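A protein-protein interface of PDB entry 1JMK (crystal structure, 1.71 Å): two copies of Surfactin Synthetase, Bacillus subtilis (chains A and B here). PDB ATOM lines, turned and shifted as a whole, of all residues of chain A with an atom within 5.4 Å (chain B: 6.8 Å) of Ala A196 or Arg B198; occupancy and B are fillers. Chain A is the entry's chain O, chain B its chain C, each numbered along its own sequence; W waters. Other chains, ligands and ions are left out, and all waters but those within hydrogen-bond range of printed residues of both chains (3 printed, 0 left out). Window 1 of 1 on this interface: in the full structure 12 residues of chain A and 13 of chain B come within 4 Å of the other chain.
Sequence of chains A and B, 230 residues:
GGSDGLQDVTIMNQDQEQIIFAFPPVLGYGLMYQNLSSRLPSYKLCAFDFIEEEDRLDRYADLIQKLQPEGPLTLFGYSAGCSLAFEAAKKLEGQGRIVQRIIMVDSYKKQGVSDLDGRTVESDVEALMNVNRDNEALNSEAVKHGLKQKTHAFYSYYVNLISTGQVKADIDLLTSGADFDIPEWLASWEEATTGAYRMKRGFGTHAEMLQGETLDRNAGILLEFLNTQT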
ATOM      1  N   ALA A 169      12.426   6.929  25.235  1.00  0.00           N
ATOM      2  CA  ALA A 169      11.352   6.134  24.645  1.00  0.00           C
ATOM      3  C   ALA A 169      10.108   6.032  25.512  1.00  0.00           C
ATOM      4  O   ALA A 169      10.202   6.019  26.735  1.00  0.00           O
ATOM      5  CB  ALA A 169      11.860   4.726  24.342  1.00  0.00           C
ATOM      6  N   ASP A 170       8.946   5.957  24.872  1.00  0.00           N
ATOM      7  CA  ASP A 170       7.707   5.785  25.621  1.00  0.00           C
ATOM      8  C   ASP A 170       7.755   4.336  26.082  1.00  0.00           C
ATOM      9  O   ASP A 170       8.383   3.501  25.431  1.00  0.00           O
ATOM     10  CB  ASP A 170       6.470   5.968  24.739  1.00  0.00           C
ATOM     11  CG  ASP A 170       6.234   7.412  24.332  1.00  0.00           C
ATOM     12  OD1 ASP A 170       6.717   8.330  25.029  1.00  0.00           O
ATOM     13  OD2 ASP A 170       5.545   7.616  23.313  1.00  0.00           O
ATOM     14  N   ILE A 171       7.098   4.039  27.196  1.00  0.00           N
ATOM     15  CA  ILE A 171       7.062   2.675  27.719  1.00  0.00           C
ATOM     16  C   ILE A 171       5.607   2.266  27.916  1.00  0.00           C
ATOM     17  O   ILE A 171       4.840   2.975  28.567  1.00  0.00           O
ATOM     18  CB  ILE A 171       7.813   2.577  29.075  1.00  0.00           C
ATOM     19  CG1 ILE A 171       9.309   2.838  28.863  1.00  0.00           C
ATOM     20  CG2 ILE A 171       7.590   1.202  29.705  1.00  0.00           C
ATOM     21  CD1 ILE A 171      10.121   2.892  30.168  1.00  0.00           C
ATOM     22  N   ASP A 172       5.221   1.138  27.323  1.00  0.00           N
ATOM     23  CA  ASP A 172       3.861   0.632  27.459  1.00  0.00           C
ATOM     24  C   ASP A 172       3.952  -0.657  28.266  1.00  0.00           C
ATOM     25  O   ASP A 172       4.802  -1.500  27.985  1.00  0.00           O
ATOM     26  CB  ASP A 172       3.241   0.330  26.088  1.00  0.00           C
ATOM     27  CG  ASP A 172       3.100   1.561  25.218  1.00  0.00           C
ATOM     28  OD1 ASP A 172       2.768   2.639  25.754  1.00  0.00           O
ATOM     29  OD2 ASP A 172       3.304   1.449  23.988  1.00  0.00           O
ATOM     30  N   THR A 193      11.454   6.709  32.284  1.00  0.00           N
ATOM     31  CA  THR A 193      11.337   7.361  30.983  1.00  0.00           C
ATOM     32  C   THR A 193      10.964   8.832  31.103  1.00  0.00           C
ATOM     33  O   THR A 193      10.234   9.217  32.012  1.00  0.00           O
ATOM     34  CB  THR A 193      10.262   6.670  30.098  1.00  0.00           C
ATOM     35  OG1 THR A 193      10.118   7.390  28.867  1.00  0.00           O
ATOM     36  CG2 THR A 193       8.914   6.635  30.805  1.00  0.00           C
ATOM     37  N   THR A 194      11.475   9.647  30.187  1.00  0.00           N
ATOM     38  CA  THR A 194      11.150  11.067  30.172  1.00  0.00           C
ATOM     39  C   THR A 194       9.993  11.233  29.190  1.00  0.00           C
ATOM     40  O   THR A 194       9.492  12.336  28.969  1.00  0.00           O
ATOM     41  CB  THR A 194      12.354  11.932  29.722  1.00  0.00           C
ATOM     42  OG1 THR A 194      12.760  11.559  28.399  1.00  0.00           O
ATOM     43  CG2 THR A 194      13.513  11.751  30.675  1.00  0.00           C
ATOM     44  N   GLY A 195       9.582  10.112  28.601  1.00  0.00           N
ATOM     45  CA  GLY A 195       8.470  10.110  27.672  1.00  0.00           C
ATOM     46  C   GLY A 195       7.209   9.747  28.436  1.00  0.00           C
ATOM     47  O   GLY A 195       7.104  10.021  29.632  1.00  0.00           O
ATOM     48  N   ALA A 196       6.253   9.123  27.757  1.00  0.00           N
ATOM     49  CA  ALA A 196       5.005   8.735  28.403  1.00  0.00           C
ATOM     50  C   ALA A 196       5.058   7.290  28.880  1.00  0.00           C
ATOM     51  O   ALA A 196       5.650   6.435  28.221  1.00  0.00           O
ATOM     52  CB  ALA A 196       3.849   8.911  27.434  1.00  0.00           C
ATOM     53  N   TYR A 197       4.448   7.034  30.034  1.00  0.00           N
ATOM     54  CA  TYR A 197       4.386   5.692  30.609  1.00  0.00           C
ATOM     55  C   TYR A 197       2.917   5.316  30.569  1.00  0.00           C
ATOM     56  O   TYR A 197       2.077   5.999  31.154  1.00  0.00           O
ATOM     57  CB  TYR A 197       4.902   5.704  32.048  1.00  0.00           C
ATOM     58  CG  TYR A 197       4.746   4.393  32.796  1.00  0.00           C
ATOM     59  CD1 TYR A 197       5.000   3.169  32.169  1.00  0.00           C
ATOM     60  CD2 TYR A 197       4.415   4.382  34.147  1.00  0.00           C
ATOM     61  CE1 TYR A 197       4.935   1.969  32.876  1.00  0.00           C
ATOM     62  CE2 TYR A 197       4.349   3.186  34.870  1.00  0.00           C
ATOM     63  CZ  TYR A 197       4.615   1.987  34.225  1.00  0.00           C
ATOM     64  OH  TYR A 197       4.602   0.808  34.936  1.00  0.00           O
ATOM     65  N   ARG A 198       2.615   4.229  29.873  1.00  0.00           N
ATOM     66  CA  ARG A 198       1.242   3.781  29.715  1.00  0.00           C
ATOM     67  C   ARG A 198       1.090   2.341  30.184  1.00  0.00           C
ATOM     68  O   ARG A 198       1.973   1.518  29.963  1.00  0.00           O
ATOM     69  CB  ARG A 198       0.871   3.895  28.240  1.00  0.00           C
ATOM     70  CG  ARG A 198      -0.506   3.421  27.842  1.00  0.00           C
ATOM     71  CD  ARG A 198      -0.615   3.544  26.326  1.00  0.00           C
ATOM     72  NE  ARG A 198      -1.878   3.056  25.790  1.00  0.00           N
ATOM     73  CZ  ARG A 198      -2.145   2.981  24.490  1.00  0.00           C
ATOM     74  NH1 ARG A 198      -1.231   3.364  23.605  1.00  0.00           N
ATOM     75  NH2 ARG A 198      -3.319   2.522  24.074  1.00  0.00           N
ATOM     76  N   MET A 199      -0.024   2.046  30.842  1.00  0.00           N
ATOM     77  CA  MET A 199      -0.276   0.690  31.315  1.00  0.00           C
ATOM     78  C   MET A 199      -1.737   0.321  31.103  1.00  0.00           C
ATOM     79  O   MET A 199      -2.619   1.183  31.107  1.00  0.00           O
ATOM     80  CB  MET A 199       0.068   0.571  32.799  1.00  0.00           C
ATOM     81  CG  MET A 199      -0.801   1.421  33.703  1.00  0.00           C
ATOM     82  SD  MET A 199      -0.189   1.432  35.386  1.00  0.00           S
ATOM     83  CE  MET A 199       1.043   2.702  35.289  1.00  0.00           C
ATOM     84  N   THR A 228      -0.522   2.954  18.148  1.00  0.00           N
ATOM     85  CA  THR A 228      -0.650   4.285  18.729  1.00  0.00           C
ATOM     86  C   THR A 228       0.168   5.327  17.980  1.00  0.00           C
ATOM     87  O   THR A 228       1.354   5.133  17.711  1.00  0.00           O
ATOM     88  CB  THR A 228      -0.215   4.292  20.204  1.00  0.00           C
ATOM     89  OG1 THR A 228      -1.116   3.481  20.966  1.00  0.00           O
ATOM     90  CG2 THR A 228      -0.217   5.713  20.760  1.00  0.00           C
ATOM     91  N   ARG B 101     -11.756   9.591  26.739  1.00  0.00           N
ATOM     92  CA  ARG B 101     -10.635   9.786  27.636  1.00  0.00           C
ATOM     93  C   ARG B 101     -10.872  10.921  28.611  1.00  0.00           C
ATOM     94  O   ARG B 101     -11.686  11.809  28.361  1.00  0.00           O
ATOM     95  CB  ARG B 101      -9.370  10.089  26.830  1.00  0.00           C
ATOM     96  CG  ARG B 101      -9.338  11.489  26.257  1.00  0.00           C
ATOM     97  CD  ARG B 101      -7.930  11.889  25.824  1.00  0.00           C
ATOM     98  NE  ARG B 101      -7.596  11.384  24.497  1.00  0.00           N
ATOM     99  CZ  ARG B 101      -8.240  11.733  23.386  1.00  0.00           C
ATOM    100  NH1 ARG B 101      -7.870  11.228  22.218  1.00  0.00           N
ATOM    101  NH2 ARG B 101      -9.258  12.588  23.442  1.00  0.00           N
ATOM    102  N   ILE B 103      -8.485  13.629  30.764  1.00  0.00           N
ATOM    103  CA  ILE B 103      -7.130  14.141  30.939  1.00  0.00           C
ATOM    104  C   ILE B 103      -7.089  14.785  32.317  1.00  0.00           C
ATOM    105  O   ILE B 103      -7.909  15.653  32.625  1.00  0.00           O
ATOM    106  CB  ILE B 103      -6.789  15.166  29.838  1.00  0.00           C
ATOM    107  CG1 ILE B 103      -6.702  14.442  28.492  1.00  0.00           C
ATOM    108  CG2 ILE B 103      -5.473  15.864  30.159  1.00  0.00           C
ATOM    109  CD1 ILE B 103      -6.592  15.352  27.299  1.00  0.00           C
ATOM    110  N   ASP B 170     -10.018   5.987  28.720  1.00  0.00           N
ATOM    111  CA  ASP B 170      -8.580   5.989  28.967  1.00  0.00           C
ATOM    112  C   ASP B 170      -8.368   7.180  29.883  1.00  0.00           C
ATOM    113  O   ASP B 170      -9.162   8.119  29.869  1.00  0.00           O
ATOM    114  CB  ASP B 170      -7.782   6.223  27.682  1.00  0.00           C
ATOM    115  CG  ASP B 170      -7.839   5.047  26.724  1.00  0.00           C
ATOM    116  OD1 ASP B 170      -8.055   3.901  27.175  1.00  0.00           O
ATOM    117  OD2 ASP B 170      -7.646   5.273  25.513  1.00  0.00           O
ATOM    118  N   ILE B 171      -7.304   7.144  30.674  1.00  0.00           N
ATOM    119  CA  ILE B 171      -7.011   8.246  31.579  1.00  0.00           C
ATOM    120  C   ILE B 171      -5.567   8.664  31.360  1.00  0.00           C
ATOM    121  O   ILE B 171      -4.659   7.831  31.425  1.00  0.00           O
ATOM    122  CB  ILE B 171      -7.200   7.830  33.062  1.00  0.00           C
ATOM    123  CG1 ILE B 171      -8.680   7.542  33.343  1.00  0.00           C
ATOM    124  CG2 ILE B 171      -6.681   8.937  33.991  1.00  0.00           C
ATOM    125  CD1 ILE B 171      -8.951   7.017  34.762  1.00  0.00           C
ATOM    126  N   ASP B 172      -5.367   9.950  31.076  1.00  0.00           N
ATOM    127  CA  ASP B 172      -4.031  10.505  30.873  1.00  0.00           C
ATOM    128  C   ASP B 172      -3.758  11.460  32.023  1.00  0.00           C
ATOM    129  O   ASP B 172      -4.587  12.321  32.326  1.00  0.00           O
ATOM    130  CB  ASP B 172      -3.938  11.299  29.569  1.00  0.00           C
ATOM    131  CG  ASP B 172      -4.142  10.448  28.339  1.00  0.00           C
ATOM    132  OD1 ASP B 172      -3.596   9.327  28.287  1.00  0.00           O
ATOM    133  OD2 ASP B 172      -4.838  10.915  27.414  1.00  0.00           O
ATOM    134  N   LEU B 173      -2.590  11.321  32.642  1.00  0.00           N
ATOM    135  CA  LEU B 173      -2.220  12.162  33.769  1.00  0.00           C
ATOM    136  C   LEU B 173      -0.920  12.924  33.532  1.00  0.00           C
ATOM    137  O   LEU B 173       0.107  12.329  33.212  1.00  0.00           O
ATOM    138  CB  LEU B 173      -2.070  11.301  35.032  1.00  0.00           C
ATOM    139  CG  LEU B 173      -1.473  11.965  36.283  1.00  0.00           C
ATOM    140  CD1 LEU B 173      -2.468  12.980  36.849  1.00  0.00           C
ATOM    141  CD2 LEU B 173      -1.164  10.904  37.332  1.00  0.00           C
ATOM    142  N   LEU B 174      -0.986  14.243  33.683  1.00  0.00           N
ATOM    143  CA  LEU B 174       0.194  15.095  33.556  1.00  0.00           C
ATOM    144  C   LEU B 174       0.617  15.329  35.002  1.00  0.00           C
ATOM    145  O   LEU B 174      -0.137  15.912  35.776  1.00  0.00           O
ATOM    146  CB  LEU B 174      -0.170  16.433  32.888  1.00  0.00           C
ATOM    147  CG  LEU B 174       0.961  17.476  32.823  1.00  0.00           C
ATOM    148  CD1 LEU B 174       2.085  16.979  31.931  1.00  0.00           C
ATOM    149  CD2 LEU B 174       0.406  18.782  32.277  1.00  0.00           C
ATOM    150  N   ALA B 196      -6.660   2.348  29.089  1.00  0.00           N
ATOM    151  CA  ALA B 196      -5.239   2.604  29.291  1.00  0.00           C
ATOM    152  C   ALA B 196      -5.032   3.774  30.235  1.00  0.00           C
ATOM    153  O   ALA B 196      -5.766   4.762  30.177  1.00  0.00           O
ATOM    154  CB  ALA B 196      -4.570   2.896  27.961  1.00  0.00           C
ATOM    155  N   TYR B 197      -4.033   3.653  31.102  1.00  0.00           N
ATOM    156  CA  TYR B 197      -3.683   4.707  32.050  1.00  0.00           C
ATOM    157  C   TYR B 197      -2.309   5.200  31.615  1.00  0.00           C
ATOM    158  O   TYR B 197      -1.342   4.444  31.620  1.00  0.00           O
ATOM    159  CB  TYR B 197      -3.626   4.146  33.473  1.00  0.00           C
ATOM    160  CG  TYR B 197      -3.150   5.125  34.531  1.00  0.00           C
ATOM    161  CD1 TYR B 197      -3.533   6.466  34.500  1.00  0.00           C
ATOM    162  CD2 TYR B 197      -2.377   4.686  35.605  1.00  0.00           C
ATOM    163  CE1 TYR B 197      -3.164   7.344  35.519  1.00  0.00           C
ATOM    164  CE2 TYR B 197      -2.004   5.555  36.634  1.00  0.00           C
ATOM    165  CZ  TYR B 197      -2.407   6.880  36.584  1.00  0.00           C
ATOM    166  OH  TYR B 197      -2.085   7.724  37.622  1.00  0.00           O
ATOM    167  N   ARG B 198      -2.226   6.466  31.232  1.00  0.00           N
ATOM    168  CA  ARG B 198      -0.959   7.016  30.765  1.00  0.00           C
ATOM    169  C   ARG B 198      -0.558   8.220  31.589  1.00  0.00           C
ATOM    170  O   ARG B 198      -1.413   8.991  32.023  1.00  0.00           O
ATOM    171  CB  ARG B 198      -1.085   7.414  29.294  1.00  0.00           C
ATOM    172  CG  ARG B 198       0.112   8.168  28.733  1.00  0.00           C
ATOM    173  CD  ARG B 198      -0.007   8.365  27.225  1.00  0.00           C
ATOM    174  NE  ARG B 198      -1.260   9.009  26.842  1.00  0.00           N
ATOM    175  CZ  ARG B 198      -1.556   9.387  25.602  1.00  0.00           C
ATOM    176  NH1 ARG B 198      -0.686   9.188  24.619  1.00  0.00           N
ATOM    177  NH2 ARG B 198      -2.725   9.952  25.341  1.00  0.00           N
ATOM    178  N   MET B 199       0.740   8.362  31.823  1.00  0.00           N
ATOM    179  CA  MET B 199       1.246   9.501  32.581  1.00  0.00           C
ATOM    180  C   MET B 199       2.548  10.006  31.973  1.00  0.00           C
ATOM    181  O   MET B 199       3.304   9.248  31.364  1.00  0.00           O
ATOM    182  CB  MET B 199       1.488   9.102  34.038  1.00  0.00           C
ATOM    183  CG  MET B 199       2.530   8.015  34.215  1.00  0.00           C
ATOM    184  SD  MET B 199       2.542   7.361  35.891  1.00  0.00           S
ATOM    185  CE  MET B 199       1.256   6.199  35.798  1.00  0.00           C
ATOM    186  N   LYS B 200       2.784  11.304  32.113  1.00  0.00           N
ATOM    187  CA  LYS B 200       4.015  11.907  31.624  1.00  0.00           C
ATOM    188  C   LYS B 200       4.329  13.038  32.580  1.00  0.00           C
ATOM    189  O   LYS B 200       3.420  13.744  33.029  1.00  0.00           O
ATOM    190  CB  LYS B 200       3.865  12.444  30.199  1.00  0.00           C
ATOM    191  CG  LYS B 200       5.185  12.978  29.635  1.00  0.00           C
ATOM    192  CD  LYS B 200       5.137  13.135  28.121  1.00  0.00           C
ATOM    193  CE  LYS B 200       6.451  13.694  27.578  1.00  0.00           C
ATOM    194  NZ  LYS B 200       6.472  13.685  26.087  1.00  0.00           N
ATOM    195  N   ARG B 201       5.609  13.185  32.910  1.00  0.00           N
ATOM    196  CA  ARG B 201       6.049  14.224  33.834  1.00  0.00           C
ATOM    197  C   ARG B 201       6.052  15.584  33.154  1.00  0.00           C
ATOM    198  O   ARG B 201       6.619  15.753  32.072  1.00  0.00           O
ATOM    199  CB  ARG B 201       7.450  13.898  34.371  1.00  0.00           C
ATOM    200  CG  ARG B 201       8.000  14.933  35.354  1.00  0.00           C
ATOM    201  CD  ARG B 201       9.165  14.369  36.159  1.00  0.00           C
ATOM    202  NE  ARG B 201       9.794  15.378  37.010  1.00  0.00           N
ATOM    203  CZ  ARG B 201      10.791  16.172  36.628  1.00  0.00           C
ATOM    204  NH1 ARG B 201      11.293  17.064  37.474  1.00  0.00           N
ATOM    205  NH2 ARG B 201      11.305  16.065  35.408  1.00  0.00           N
ATOM    206  N   GLU B 224      -0.111  16.532  23.213  1.00  0.00           N
ATOM    207  CA  GLU B 224       0.348  15.198  22.837  1.00  0.00           C
ATOM    208  C   GLU B 224      -0.739  14.203  23.243  1.00  0.00           C
ATOM    209  O   GLU B 224      -1.086  13.301  22.479  1.00  0.00           O
ATOM    210  CB  GLU B 224       1.657  14.848  23.551  1.00  0.00           C
ATOM    211  CG  GLU B 224       2.866  15.622  23.057  1.00  0.00           C
ATOM    212  CD  GLU B 224       4.128  15.307  23.847  1.00  0.00           C
ATOM    213  OE1 GLU B 224       5.190  15.877  23.518  1.00  0.00           O
ATOM    214  OE2 GLU B 224       4.065  14.495  24.795  1.00  0.00           O
ATOM    215  N   PHE B 225      -1.276  14.369  24.449  1.00  0.00           N
ATOM    216  CA  PHE B 225      -2.330  13.480  24.927  1.00  0.00           C
ATOM    217  C   PHE B 225      -3.542  13.562  24.011  1.00  0.00           C
ATOM    218  O   PHE B 225      -4.081  12.545  23.585  1.00  0.00           O
ATOM    219  CB  PHE B 225      -2.791  13.855  26.344  1.00  0.00           C
ATOM    220  CG  PHE B 225      -1.787  13.570  27.428  1.00  0.00           C
ATOM    221  CD1 PHE B 225      -0.783  12.626  27.251  1.00  0.00           C
ATOM    222  CD2 PHE B 225      -1.893  14.209  28.661  1.00  0.00           C
ATOM    223  CE1 PHE B 225       0.097  12.320  28.292  1.00  0.00           C
ATOM    224  CE2 PHE B 225      -1.022  13.910  29.704  1.00  0.00           C
ATOM    225  CZ  PHE B 225      -0.026  12.962  29.520  1.00  0.00           C
ATOM    226  N   LEU B 226      -3.968  14.786  23.720  1.00  0.00           N
ATOM    227  CA  LEU B 226      -5.139  15.017  22.882  1.00  0.00           C
ATOM    228  C   LEU B 226      -4.999  14.537  21.445  1.00  0.00           C
ATOM    229  O   LEU B 226      -5.967  14.050  20.854  1.00  0.00           O
ATOM    230  CB  LEU B 226      -5.485  16.507  22.881  1.00  0.00           C
ATOM    231  CG  LEU B 226      -6.092  17.081  24.158  1.00  0.00           C
ATOM    232  CD1 LEU B 226      -5.992  18.599  24.124  1.00  0.00           C
ATOM    233  CD2 LEU B 226      -7.550  16.632  24.290  1.00  0.00           C
ATOM    234  N   ASN B 227      -3.803  14.681  20.883  1.00  0.00           N
ATOM    235  CA  ASN B 227      -3.549  14.287  19.502  1.00  0.00           C
ATOM    236  C   ASN B 227      -3.184  12.814  19.351  1.00  0.00           C
ATOM    237  O   ASN B 227      -2.647  12.407  18.321  1.00  0.00           O
ATOM    238  CB  ASN B 227      -2.440  15.163  18.908  1.00  0.00           C
ATOM    239  CG  ASN B 227      -2.835  16.633  18.818  1.00  0.00           C
ATOM    240  OD1 ASN B 227      -1.979  17.510  18.687  1.00  0.00           O
ATOM    241  ND2 ASN B 227      -4.134  16.907  18.878  1.00  0.00           N
ATOM    242  N   THR B 228      -3.473  12.016  20.375  1.00  0.00           N
ATOM    243  CA  THR B 228      -3.179  10.587  20.330  1.00  0.00           C
ATOM    244  C   THR B 228      -4.384   9.820  19.792  1.00  0.00           C
ATOM    245  O   THR B 228      -5.534  10.181  20.054  1.00  0.00           O
ATOM    246  CB  THR B 228      -2.828  10.041  21.729  1.00  0.00           C
ATOM    247  OG1 THR B 228      -1.641  10.682  22.209  1.00  0.00           O
ATOM    248  CG2 THR B 228      -2.594   8.534  21.672  1.00  0.00           C
ATOM    249  N   GLN B 229      -4.115   8.762  19.035  1.00  0.00           N
ATOM    250  CA  GLN B 229      -5.177   7.946  18.463  1.00  0.00           C
ATOM    251  C   GLN B 229      -4.677   6.533  18.192  1.00  0.00           C
ATOM    252  O   GLN B 229      -3.471   6.285  18.160  1.00  0.00           O
ATOM    253  CB  GLN B 229      -5.683   8.579  17.170  1.00  0.00           C
HETATM  254  O   HOH W   1       6.039  11.118  24.849  1.00  0.00           O
HETATM  255  O   HOH W   2       7.567  11.282  31.900  1.00  0.00           O
HETATM  256  O   HOH W   3       8.770  14.336  30.637  1.00  0.00           O
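Of the 19 printed residues of chain B, 7 touch a printed residue of chain A.
Printed residues of chain B that touch a printed residue of chain A: Ala B196, Tyr B197, Arg B198, Met B199, Lys B200, Thr B228 and Gln B229.
Hydrophobic or aromatic side chains of chain B within 4 Å of the printed part of chain A: Ala B196, Tyr B197 and Met B199.
Of the 12 printed residues of chain A, 7 touch a printed residue of chain B.
Printed residues of chain A that touch a printed residue of chain B: Thr A194, Gly A195, Ala A196, Tyr A197, Arg A198, Met A199 and Thr A228.
Along chain A the printed residues that touch a printed residue of chain B span positions 194 to 228.
Among the printed residues, no Asp or Glu carboxylate lies within 4 Å of a Lys or Arg side-chain nitrogen of the other chain.
The backbone NH (N) of Met A199 is in hydrogen-bond range of the backbone carbonyl oxygen (O) of Tyr B197 (2.8 Å).
The backbone NH (N) of Met B199 sits at hydrogen-bond distance from the backbone carbonyl oxygen (O) of Tyr A197, at 2.8 Å.
N of Arg B198 lies within hydrogen-bond range of O of Ile B171.
O of Leu B173 lies within hydrogen-bond range of N of Lys B200 (3.1 Å).
O of Phe B225 sits at hydrogen-bond distance from NH2 of Arg B198, at 3.4 Å.
The side-chain amino group of Lys B200 lies within salt-bridge range of the side-chain carboxylate of Glu B224 (2.8 Å).
The backbone carbonyl oxygen (O) of Glu B224 sits at hydrogen-bond distance from the side-chain hydroxyl (OG1) of Thr B228 (2.7 Å).
The backbone NH (N) of Ile A171 sits at hydrogen-bond distance from the backbone carbonyl oxygen (O) of Ala A196, at 3.0 Å.
Water W2 lies within hydrogen-bond range of O of Gly A195 (2.6 Å), N of Arg B201 (2.9 Å) and O of Thr A193 (3.4 Å).
Water W3 bridges the backbone carbonyl oxygen of Thr A194 (2.7 Å) and the backbone carbonyl oxygen of Arg B201 (2.9 Å).
Water W1 bridges OD1 of Asp A170 (2.9 Å) and NZ of Lys B200 (2.9 Å).
Of the printed residues of chain B, Ala A196 touches Arg B198 (3.9 Å) and Met B199 (3.5 Å).
Of chain A, only Ala A196 and Tyr A197 come within 4 Å of Arg B198.
Printed residues of chain A within 4 Å of Tyr B197: Tyr A197, Arg A198 and Met A199.
Printed residues of chain A within 4 Å of Thr B228: Thr A228.
Of the printed residues of chain B, Thr A194 touches Lys B200.
Of the printed residues of chain B, Met A199 touches Ala B196 (3.5 Å), Tyr B197 (2.8 Å) and Met B199 (3.5 Å).
The nearest residue of chain B that does not touch Ala A196 is Lys B200 (4.2 Å).
The nearest residue of chain A that does not touch Arg B198 is Arg A198 (4.1 Å).
The nearest printed residue of chain B that does not touch Tyr A197 is Lys B200 (5.0 Å).
Ala A196 touches Met B199, and with the chains exchanged Met A199 touches Ala B196.
Tyr A197 touches its own counterpart, Tyr B197.
Tyr A197 touches Arg B198, and with the chains exchanged Arg A198 touches Tyr B197.
Thr B228 touches its own counterpart, Thr A228.
8 positions are printed for both chains.
Of the 14 pairs that touch across the chains among the printed residues, 11 have their exchanged pair printed and touching as well.
Among the printed residues, merely in contact across the chains: Tyr A197 with Arg B198, Arg A198 with Tyr B197, Ala A196 with Met B199, Arg A198 with Ala B196, Met A199 with Ala B196, Thr A228 with Gln B229, Gly A195 with Lys B200, Met A199 with Met B199, Thr A194 with Lys B200, Tyr A197 with Tyr B197, Thr A228 with Thr B228 and Ala A196 with Arg B198.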
